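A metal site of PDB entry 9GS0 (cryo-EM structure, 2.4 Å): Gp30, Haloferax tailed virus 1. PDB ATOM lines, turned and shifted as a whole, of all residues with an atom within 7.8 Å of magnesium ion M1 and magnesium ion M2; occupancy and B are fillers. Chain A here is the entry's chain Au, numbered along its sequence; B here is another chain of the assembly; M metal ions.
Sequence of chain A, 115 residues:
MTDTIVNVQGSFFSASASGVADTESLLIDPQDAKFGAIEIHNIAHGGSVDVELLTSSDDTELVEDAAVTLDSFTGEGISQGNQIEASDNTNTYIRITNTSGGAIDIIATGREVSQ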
ATOM      1  N   ASP A  29      32.183  -7.494 -25.958  1.00  0.00           N
ATOM      2  CA  ASP A  29      31.294  -8.632 -25.780  1.00  0.00           C
ATOM      3  C   ASP A  29      31.711  -9.399 -24.529  1.00  0.00           C
ATOM      4  O   ASP A  29      32.826  -9.903 -24.471  1.00  0.00           O
ATOM      5  CB  ASP A  29      31.327  -9.502 -27.041  1.00  0.00           C
ATOM      6  CG  ASP A  29      30.469 -10.732 -27.013  1.00  0.00           C
ATOM      7  OD1 ASP A  29      29.850 -10.983 -26.013  1.00  0.00           O
ATOM      8  OD2 ASP A  29      30.460 -11.420 -27.997  1.00  0.00           O
ATOM      9  N   PRO A  30      30.851  -9.522 -23.496  1.00  0.00           N
ATOM     10  CA  PRO A  30      31.166 -10.312 -22.305  1.00  0.00           C
ATOM     11  C   PRO A  30      31.410 -11.807 -22.515  1.00  0.00           C
ATOM     12  O   PRO A  30      31.870 -12.475 -21.580  1.00  0.00           O
ATOM     13  CB  PRO A  30      29.936 -10.110 -21.405  1.00  0.00           C
ATOM     14  CG  PRO A  30      29.354  -8.813 -21.867  1.00  0.00           C
ATOM     15  CD  PRO A  30      29.574  -8.831 -23.356  1.00  0.00           C
ATOM     16  N   GLN A  31      31.142 -12.338 -23.713  1.00  0.00           N
ATOM     17  CA  GLN A  31      31.461 -13.714 -24.060  1.00  0.00           C
ATOM     18  C   GLN A  31      32.963 -13.951 -24.020  1.00  0.00           C
ATOM     19  O   GLN A  31      33.395 -15.079 -23.823  1.00  0.00           O
ATOM     20  CB  GLN A  31      30.929 -14.097 -25.450  1.00  0.00           C
ATOM     21  CG  GLN A  31      29.447 -14.392 -25.494  1.00  0.00           C
ATOM     22  CD  GLN A  31      28.906 -14.713 -26.852  1.00  0.00           C
ATOM     23  OE1 GLN A  31      28.458 -15.783 -27.121  1.00  0.00           O
ATOM     24  NE2 GLN A  31      28.978 -13.765 -27.739  1.00  0.00           N
ATOM     25  N   GLY A  36      32.183 -14.397 -17.705  1.00  0.00           N
ATOM     26  CA  GLY A  36      30.955 -14.201 -18.459  1.00  0.00           C
ATOM     27  C   GLY A  36      30.388 -12.778 -18.375  1.00  0.00           C
ATOM     28  O   GLY A  36      29.517 -12.427 -19.165  1.00  0.00           O
ATOM     29  N   SER A  56      20.722  -7.561 -26.634  1.00  0.00           N
ATOM     30  CA  SER A  56      20.434  -8.397 -27.792  1.00  0.00           C
ATOM     31  C   SER A  56      19.159  -9.215 -27.565  1.00  0.00           C
ATOM     32  O   SER A  56      18.845  -9.566 -26.440  1.00  0.00           O
ATOM     33  CB  SER A  56      21.577  -9.302 -28.114  1.00  0.00           C
ATOM     34  OG  SER A  56      21.298 -10.062 -29.274  1.00  0.00           O
ATOM     35  N   ASP A  58      19.130 -12.123 -29.128  1.00  0.00           N
ATOM     36  CA  ASP A  58      19.740 -13.433 -29.310  1.00  0.00           C
ATOM     37  C   ASP A  58      20.831 -13.634 -28.272  1.00  0.00           C
ATOM     38  O   ASP A  58      21.538 -12.688 -27.960  1.00  0.00           O
ATOM     39  CB  ASP A  58      20.315 -13.596 -30.719  1.00  0.00           C
ATOM     40  CG  ASP A  58      20.977 -14.924 -30.989  1.00  0.00           C
ATOM     41  OD1 ASP A  58      22.035 -15.149 -30.457  1.00  0.00           O
ATOM     42  OD2 ASP A  58      20.416 -15.705 -31.722  1.00  0.00           O
ATOM     43  N   ASP A  59      20.985 -14.873 -27.780  1.00  0.00           N
ATOM     44  CA  ASP A  59      21.802 -15.223 -26.630  1.00  0.00           C
ATOM     45  C   ASP A  59      23.308 -15.082 -26.911  1.00  0.00           C
ATOM     46  O   ASP A  59      24.075 -14.869 -25.984  1.00  0.00           O
ATOM     47  CB  ASP A  59      21.405 -16.603 -26.132  1.00  0.00           C
ATOM     48  CG  ASP A  59      20.070 -16.674 -25.453  1.00  0.00           C
ATOM     49  OD1 ASP A  59      19.635 -15.744 -24.929  1.00  0.00           O
ATOM     50  OD2 ASP A  59      19.463 -17.628 -25.565  1.00  0.00           O
ATOM     51  N   THR A  60      23.695 -15.167 -28.206  1.00  0.00           N
ATOM     52  CA  THR A  60      25.057 -15.399 -28.645  1.00  0.00           C
ATOM     53  C   THR A  60      25.570 -14.328 -29.617  1.00  0.00           C
ATOM     54  O   THR A  60      26.774 -14.079 -29.648  1.00  0.00           O
ATOM     55  CB  THR A  60      25.193 -16.778 -29.286  1.00  0.00           C
ATOM     56  OG1 THR A  60      24.358 -16.816 -30.429  1.00  0.00           O
ATOM     57  CG2 THR A  60      24.852 -17.913 -28.354  1.00  0.00           C
ATOM     58  N   GLU A  61      24.683 -13.728 -30.417  1.00  0.00           N
ATOM     59  CA  GLU A  61      25.035 -12.675 -31.359  1.00  0.00           C
ATOM     60  C   GLU A  61      24.276 -11.404 -31.003  1.00  0.00           C
ATOM     61  O   GLU A  61      23.198 -11.474 -30.416  1.00  0.00           O
ATOM     62  CB  GLU A  61      24.694 -13.085 -32.799  1.00  0.00           C
ATOM     63  CG  GLU A  61      25.513 -14.205 -33.377  1.00  0.00           C
ATOM     64  CD  GLU A  61      25.367 -14.454 -34.828  1.00  0.00           C
ATOM     65  OE1 GLU A  61      24.382 -14.170 -35.367  1.00  0.00           O
ATOM     66  OE2 GLU A  61      26.241 -14.941 -35.378  1.00  0.00           O
ATOM     67  N   SER A  87      26.895  -8.219 -19.351  1.00  0.00           N
ATOM     68  CA  SER A  87      26.814  -9.641 -19.050  1.00  0.00           C
ATOM     69  C   SER A  87      26.359 -10.400 -20.285  1.00  0.00           C
ATOM     70  O   SER A  87      25.591  -9.891 -21.085  1.00  0.00           O
ATOM     71  CB  SER A  87      25.839  -9.877 -17.927  1.00  0.00           C
ATOM     72  OG  SER A  87      26.516 -10.190 -16.720  1.00  0.00           O
ATOM     73  N   ASP A  88      26.827 -11.644 -20.399  1.00  0.00           N
ATOM     74  CA  ASP A  88      26.409 -12.496 -21.498  1.00  0.00           C
ATOM     75  C   ASP A  88      25.015 -13.061 -21.218  1.00  0.00           C
ATOM     76  O   ASP A  88      24.197 -13.136 -22.149  1.00  0.00           O
ATOM     77  CB  ASP A  88      27.442 -13.576 -21.822  1.00  0.00           C
ATOM     78  CG  ASP A  88      27.078 -14.456 -22.982  1.00  0.00           C
ATOM     79  OD1 ASP A  88      26.241 -14.082 -23.774  1.00  0.00           O
ATOM     80  OD2 ASP A  88      27.663 -15.500 -23.078  1.00  0.00           O
ATOM     81  N   ASN A  89      24.741 -13.441 -19.957  1.00  0.00           N
ATOM     82  CA  ASN A  89      23.469 -14.084 -19.626  1.00  0.00           C
ATOM     83  C   ASN A  89      22.315 -13.092 -19.590  1.00  0.00           C
ATOM     84  O   ASN A  89      21.167 -13.487 -19.708  1.00  0.00           O
ATOM     85  CB  ASN A  89      23.545 -14.936 -18.353  1.00  0.00           C
ATOM     86  CG  ASN A  89      22.395 -15.903 -18.201  1.00  0.00           C
ATOM     87  OD1 ASN A  89      21.925 -16.491 -19.182  1.00  0.00           O
ATOM     88  ND2 ASN A  89      21.930 -16.117 -16.973  1.00  0.00           N
ATOM     89  N   THR A  90      22.635 -11.803 -19.432  1.00  0.00           N
ATOM     90  CA  THR A  90      21.657 -10.734 -19.556  1.00  0.00           C
ATOM     91  C   THR A  90      21.708 -10.100 -20.945  1.00  0.00           C
ATOM     92  O   THR A  90      21.005  -9.132 -21.201  1.00  0.00           O
ATOM     93  CB  THR A  90      21.787  -9.689 -18.457  1.00  0.00           C
ATOM     94  OG1 THR A  90      22.861  -8.809 -18.756  1.00  0.00           O
ATOM     95  CG2 THR A  90      22.002 -10.292 -17.096  1.00  0.00           C
ATOM     96  N   ASN A  91      22.549 -10.662 -21.839  1.00  0.00           N
ATOM     97  CA  ASN A  91      22.687 -10.306 -23.249  1.00  0.00           C
ATOM     98  C   ASN A  91      22.975  -8.819 -23.476  1.00  0.00           C
ATOM     99  O   ASN A  91      22.442  -8.229 -24.411  1.00  0.00           O
ATOM    100  CB  ASN A  91      21.536 -10.867 -24.088  1.00  0.00           C
ATOM    101  CG  ASN A  91      21.563 -12.373 -24.147  1.00  0.00           C
ATOM    102  OD1 ASN A  91      22.586 -12.982 -24.301  1.00  0.00           O
ATOM    103  ND2 ASN A  91      20.427 -12.987 -23.992  1.00  0.00           N
ATOM    104  N   THR A  92      23.860  -8.220 -22.651  1.00  0.00           N
ATOM    105  CA  THR A  92      24.243  -6.823 -22.830  1.00  0.00           C
ATOM    106  C   THR A  92      25.626  -6.700 -23.471  1.00  0.00           C
ATOM    107  O   THR A  92      26.525  -7.457 -23.162  1.00  0.00           O
ATOM    108  CB  THR A  92      24.091  -5.981 -21.561  1.00  0.00           C
ATOM    109  OG1 THR A  92      24.562  -6.744 -20.458  1.00  0.00           O
ATOM    110  CG2 THR A  92      22.675  -5.545 -21.299  1.00  0.00           C
ATOM    111  N   TYR A  93      25.744  -5.705 -24.367  1.00  0.00           N
ATOM    112  CA  TYR A  93      26.937  -5.402 -25.136  1.00  0.00           C
ATOM    113  C   TYR A  93      27.239  -3.900 -25.033  1.00  0.00           C
ATOM    114  O   TYR A  93      26.316  -3.113 -24.829  1.00  0.00           O
ATOM    115  CB  TYR A  93      26.708  -5.731 -26.609  1.00  0.00           C
ATOM    116  CG  TYR A  93      26.529  -7.192 -26.950  1.00  0.00           C
ATOM    117  CD1 TYR A  93      25.353  -7.851 -26.680  1.00  0.00           C
ATOM    118  CD2 TYR A  93      27.534  -7.917 -27.564  1.00  0.00           C
ATOM    119  CE1 TYR A  93      25.190  -9.187 -26.984  1.00  0.00           C
ATOM    120  CE2 TYR A  93      27.377  -9.250 -27.874  1.00  0.00           C
ATOM    121  CZ  TYR A  93      26.202  -9.886 -27.580  1.00  0.00           C
ATOM    122  OH  TYR A  93      26.034 -11.179 -27.912  1.00  0.00           O
ATOM    123  N   GLN A 115      29.208 -13.641 -13.430  1.00  0.00           N
ATOM    124  CA  GLN A 115      27.891 -13.685 -14.039  1.00  0.00           C
ATOM    125  C   GLN A 115      26.882 -14.120 -12.988  1.00  0.00           C
ATOM    126  O   GLN A 115      27.241 -14.687 -11.990  1.00  0.00           O
ATOM    127  CB  GLN A 115      27.905 -14.685 -15.187  1.00  0.00           C
ATOM    128  CG  GLN A 115      26.626 -14.757 -15.999  1.00  0.00           C
ATOM    129  CD  GLN A 115      26.204 -13.438 -16.588  1.00  0.00           C
ATOM    130  OE1 GLN A 115      26.419 -13.140 -17.754  1.00  0.00           O
ATOM    131  NE2 GLN A 115      25.594 -12.646 -15.744  1.00  0.00           N
ATOM    132  OXT GLN A 115      25.722 -13.919 -13.155  1.00  0.00           O
ATOM    133  N   ASN B 231      15.223 -26.949 -16.626  1.00  0.00           N
ATOM    134  CA  ASN B 231      16.443 -26.232 -16.931  1.00  0.00           C
ATOM    135  C   ASN B 231      17.018 -25.713 -15.614  1.00  0.00           C
ATOM    136  O   ASN B 231      16.266 -25.244 -14.749  1.00  0.00           O
ATOM    137  CB  ASN B 231      16.140 -25.111 -17.946  1.00  0.00           C
ATOM    138  CG  ASN B 231      17.340 -24.255 -18.311  1.00  0.00           C
ATOM    139  OD1 ASN B 231      18.482 -24.701 -18.317  1.00  0.00           O
ATOM    140  ND2 ASN B 231      17.076 -23.000 -18.628  1.00  0.00           N
ATOM    141  N   ASP B 233      19.673 -22.873 -14.969  1.00  0.00           N
ATOM    142  CA  ASP B 233      20.523 -21.799 -15.463  1.00  0.00           C
ATOM    143  C   ASP B 233      21.628 -21.545 -14.438  1.00  0.00           C
ATOM    144  O   ASP B 233      21.352 -20.976 -13.366  1.00  0.00           O
ATOM    145  CB  ASP B 233      19.700 -20.525 -15.744  1.00  0.00           C
ATOM    146  CG  ASP B 233      20.468 -19.457 -16.514  1.00  0.00           C
ATOM    147  OD1 ASP B 233      21.483 -19.792 -17.141  1.00  0.00           O
ATOM    148  OD2 ASP B 233      20.041 -18.303 -16.497  1.00  0.00           O
ATOM    149  N   THR B 234      22.861 -21.966 -14.761  1.00  0.00           N
ATOM    150  CA  THR B 234      23.979 -21.804 -13.833  1.00  0.00           C
ATOM    151  C   THR B 234      24.445 -20.345 -13.769  1.00  0.00           C
ATOM    152  O   THR B 234      24.973 -19.938 -12.725  1.00  0.00           O
ATOM    153  CB  THR B 234      25.155 -22.750 -14.127  1.00  0.00           C
ATOM    154  OG1 THR B 234      25.765 -22.404 -15.380  1.00  0.00           O
ATOM    155  CG2 THR B 234      24.764 -24.210 -14.123  1.00  0.00           C
ATOM    156  N   ALA B 235      24.231 -19.572 -14.846  1.00  0.00           N
ATOM    157  CA  ALA B 235      24.711 -18.200 -14.976  1.00  0.00           C
ATOM    158  C   ALA B 235      26.219 -18.133 -14.664  1.00  0.00           C
ATOM    159  O   ALA B 235      26.629 -17.440 -13.738  1.00  0.00           O
ATOM    160  CB  ALA B 235      23.879 -17.261 -14.117  1.00  0.00           C
ATOM    161  N   SER B 334      29.770 -20.649 -23.083  1.00  0.00           N
ATOM    162  CA  SER B 334      29.102 -19.385 -23.382  1.00  0.00           C
ATOM    163  C   SER B 334      27.630 -19.494 -22.986  1.00  0.00           C
ATOM    164  O   SER B 334      27.146 -20.619 -22.802  1.00  0.00           O
ATOM    165  CB  SER B 334      29.258 -19.057 -24.858  1.00  0.00           C
ATOM    166  OG  SER B 334      28.796 -20.129 -25.664  1.00  0.00           O
ATOM    167  N   ASP B 335      26.920 -18.356 -22.867  1.00  0.00           N
ATOM    168  CA  ASP B 335      25.503 -18.299 -22.451  1.00  0.00           C
ATOM    169  C   ASP B 335      24.613 -19.183 -23.314  1.00  0.00           C
ATOM    170  O   ASP B 335      24.652 -19.093 -24.541  1.00  0.00           O
ATOM    171  CB  ASP B 335      24.983 -16.866 -22.503  1.00  0.00           C
ATOM    172  CG  ASP B 335      23.505 -16.723 -22.489  1.00  0.00           C
ATOM    173  OD1 ASP B 335      22.897 -17.505 -21.923  1.00  0.00           O
ATOM    174  OD2 ASP B 335      23.073 -15.827 -23.008  1.00  0.00           O
ATOM    175  N   GLY B 336      23.771 -19.986 -22.658  1.00  0.00           N
ATOM    176  CA  GLY B 336      22.783 -20.817 -23.334  1.00  0.00           C
ATOM    177  C   GLY B 336      23.310 -22.197 -23.762  1.00  0.00           C
ATOM    178  O   GLY B 336      22.543 -22.998 -24.295  1.00  0.00           O
ATOM    179  N   ASP B 337      24.612 -22.441 -23.525  1.00  0.00           N
ATOM    180  CA  ASP B 337      25.252 -23.726 -23.769  1.00  0.00           C
ATOM    181  C   ASP B 337      24.688 -24.774 -22.806  1.00  0.00           C
ATOM    182  O   ASP B 337      24.782 -24.613 -21.580  1.00  0.00           O
ATOM    183  CB  ASP B 337      26.771 -23.638 -23.594  1.00  0.00           C
ATOM    184  CG  ASP B 337      27.525 -22.942 -24.713  1.00  0.00           C
ATOM    185  OD1 ASP B 337      26.903 -22.638 -25.748  1.00  0.00           O
ATOM    186  OD2 ASP B 337      28.722 -22.713 -24.548  1.00  0.00           O
ATOM    187  N   LYS B 338      24.113 -25.843 -23.373  1.00  0.00           N
ATOM    188  CA  LYS B 338      23.619 -26.993 -22.615  1.00  0.00           C
ATOM    189  C   LYS B 338      24.749 -28.010 -22.500  1.00  0.00           C
ATOM    190  O   LYS B 338      25.074 -28.689 -23.473  1.00  0.00           O
ATOM    191  CB  LYS B 338      22.353 -27.569 -23.283  1.00  0.00           C
ATOM    192  CG  LYS B 338      21.211 -26.586 -23.508  1.00  0.00           C
ATOM    193  CD  LYS B 338      20.768 -25.852 -22.238  1.00  0.00           C
ATOM    194  CE  LYS B 338      19.738 -24.769 -22.489  1.00  0.00           C
ATOM    195  NZ  LYS B 338      18.431 -25.315 -22.899  1.00  0.00           N
ATOM    196  N   GLN B 395      22.683 -25.363 -17.933  1.00  0.00           N
ATOM    197  CA  GLN B 395      22.920 -24.288 -18.886  1.00  0.00           C
ATOM    198  C   GLN B 395      24.013 -23.352 -18.340  1.00  0.00           C
ATOM    199  O   GLN B 395      23.968 -22.969 -17.177  1.00  0.00           O
ATOM    200  CB  GLN B 395      21.599 -23.553 -19.150  1.00  0.00           C
ATOM    201  CG  GLN B 395      21.716 -22.345 -20.072  1.00  0.00           C
ATOM    202  CD  GLN B 395      20.391 -21.656 -20.216  1.00  0.00           C
ATOM    203  OE1 GLN B 395      19.593 -21.976 -21.089  1.00  0.00           O
ATOM    204  NE2 GLN B 395      20.140 -20.677 -19.350  1.00  0.00           N
ATOM    205  N   TYR B 396      24.982 -22.990 -19.203  1.00  0.00           N
ATOM    206  CA  TYR B 396      26.063 -22.082 -18.863  1.00  0.00           C
ATOM    207  C   TYR B 396      25.538 -20.638 -18.775  1.00  0.00           C
ATOM    208  O   TYR B 396      24.906 -20.179 -19.712  1.00  0.00           O
ATOM    209  CB  TYR B 396      27.187 -22.224 -19.906  1.00  0.00           C
ATOM    210  CG  TYR B 396      28.517 -21.578 -19.588  1.00  0.00           C
ATOM    211  CD1 TYR B 396      28.693 -20.204 -19.696  1.00  0.00           C
ATOM    212  CD2 TYR B 396      29.625 -22.353 -19.267  1.00  0.00           C
ATOM    213  CE1 TYR B 396      29.937 -19.618 -19.454  1.00  0.00           C
ATOM    214  CE2 TYR B 396      30.863 -21.784 -19.008  1.00  0.00           C
ATOM    215  CZ  TYR B 396      31.011 -20.412 -19.114  1.00  0.00           C
ATOM    216  OH  TYR B 396      32.228 -19.842 -18.860  1.00  0.00           O
ATOM    217  OXT TYR B 396      25.765 -19.930 -17.796  1.00  0.00           O
HETATM  218 MG    MG M   1      24.056 -14.164 -24.143  1.00  0.00          MG
HETATM  219 MG    MG M   2      21.084 -17.893 -20.538  1.00  0.00          MG
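The side-chain amide nitrogen (ND2) of Asn 89 is in hydrogen-bond range of the side-chain carboxylate (OD2) of Asp 233 of chain B.
The backbone carbonyl oxygen of Gln 395 of chain B is in hydrogen-bond range of the side-chain hydroxyl of Thr 234 of chain B (2.6 Å).
OD1 of Asp 233 of chain B sits at hydrogen-bond distance from NE2 of Gln 395 of chain B.
The backbone carbonyl oxygen (O) of Asn 91 sits at hydrogen-bond distance from the backbone NH (N) of Ser 56.
N of Asp 88 sits at hydrogen-bond distance from O of Gly 36 (3.1 Å).
N of Asn 89 lies within hydrogen-bond range of OE1 of Gln 115 (2.8 Å).
N of Asp 88 sits at hydrogen-bond distance from OE1 of Gln 115 (3.1 Å).
The nearest printed residue that does not touch magnesium ion M1 is Thr 60 (4.2 Å).
OD1 of Asp 233 of chain B touches magnesium ion M2, at 3.9 Å.
Gln 395 of chain B touches magnesium ion M2.
Within 4 Å of magnesium ion M2: Asn 89, Asp 233 of chain B, Asp 335 of chain B and Gln 395 of chain B.
Magnesium ion M1 is bound by OD1 of Asn 91 (1.9 Å), O of Asp 59 (2.0 Å), OD1 of Asp 88 (2.2 Å), OD2 of Asp 335 of chain B (2.2 Å) and O of Asp 88 (2.2 Å).
Magnesium ion M2 is bound by OD1 of Asn 89 (2.1 Å) and OD1 of Asp 335 of chain B (2.3 Å).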
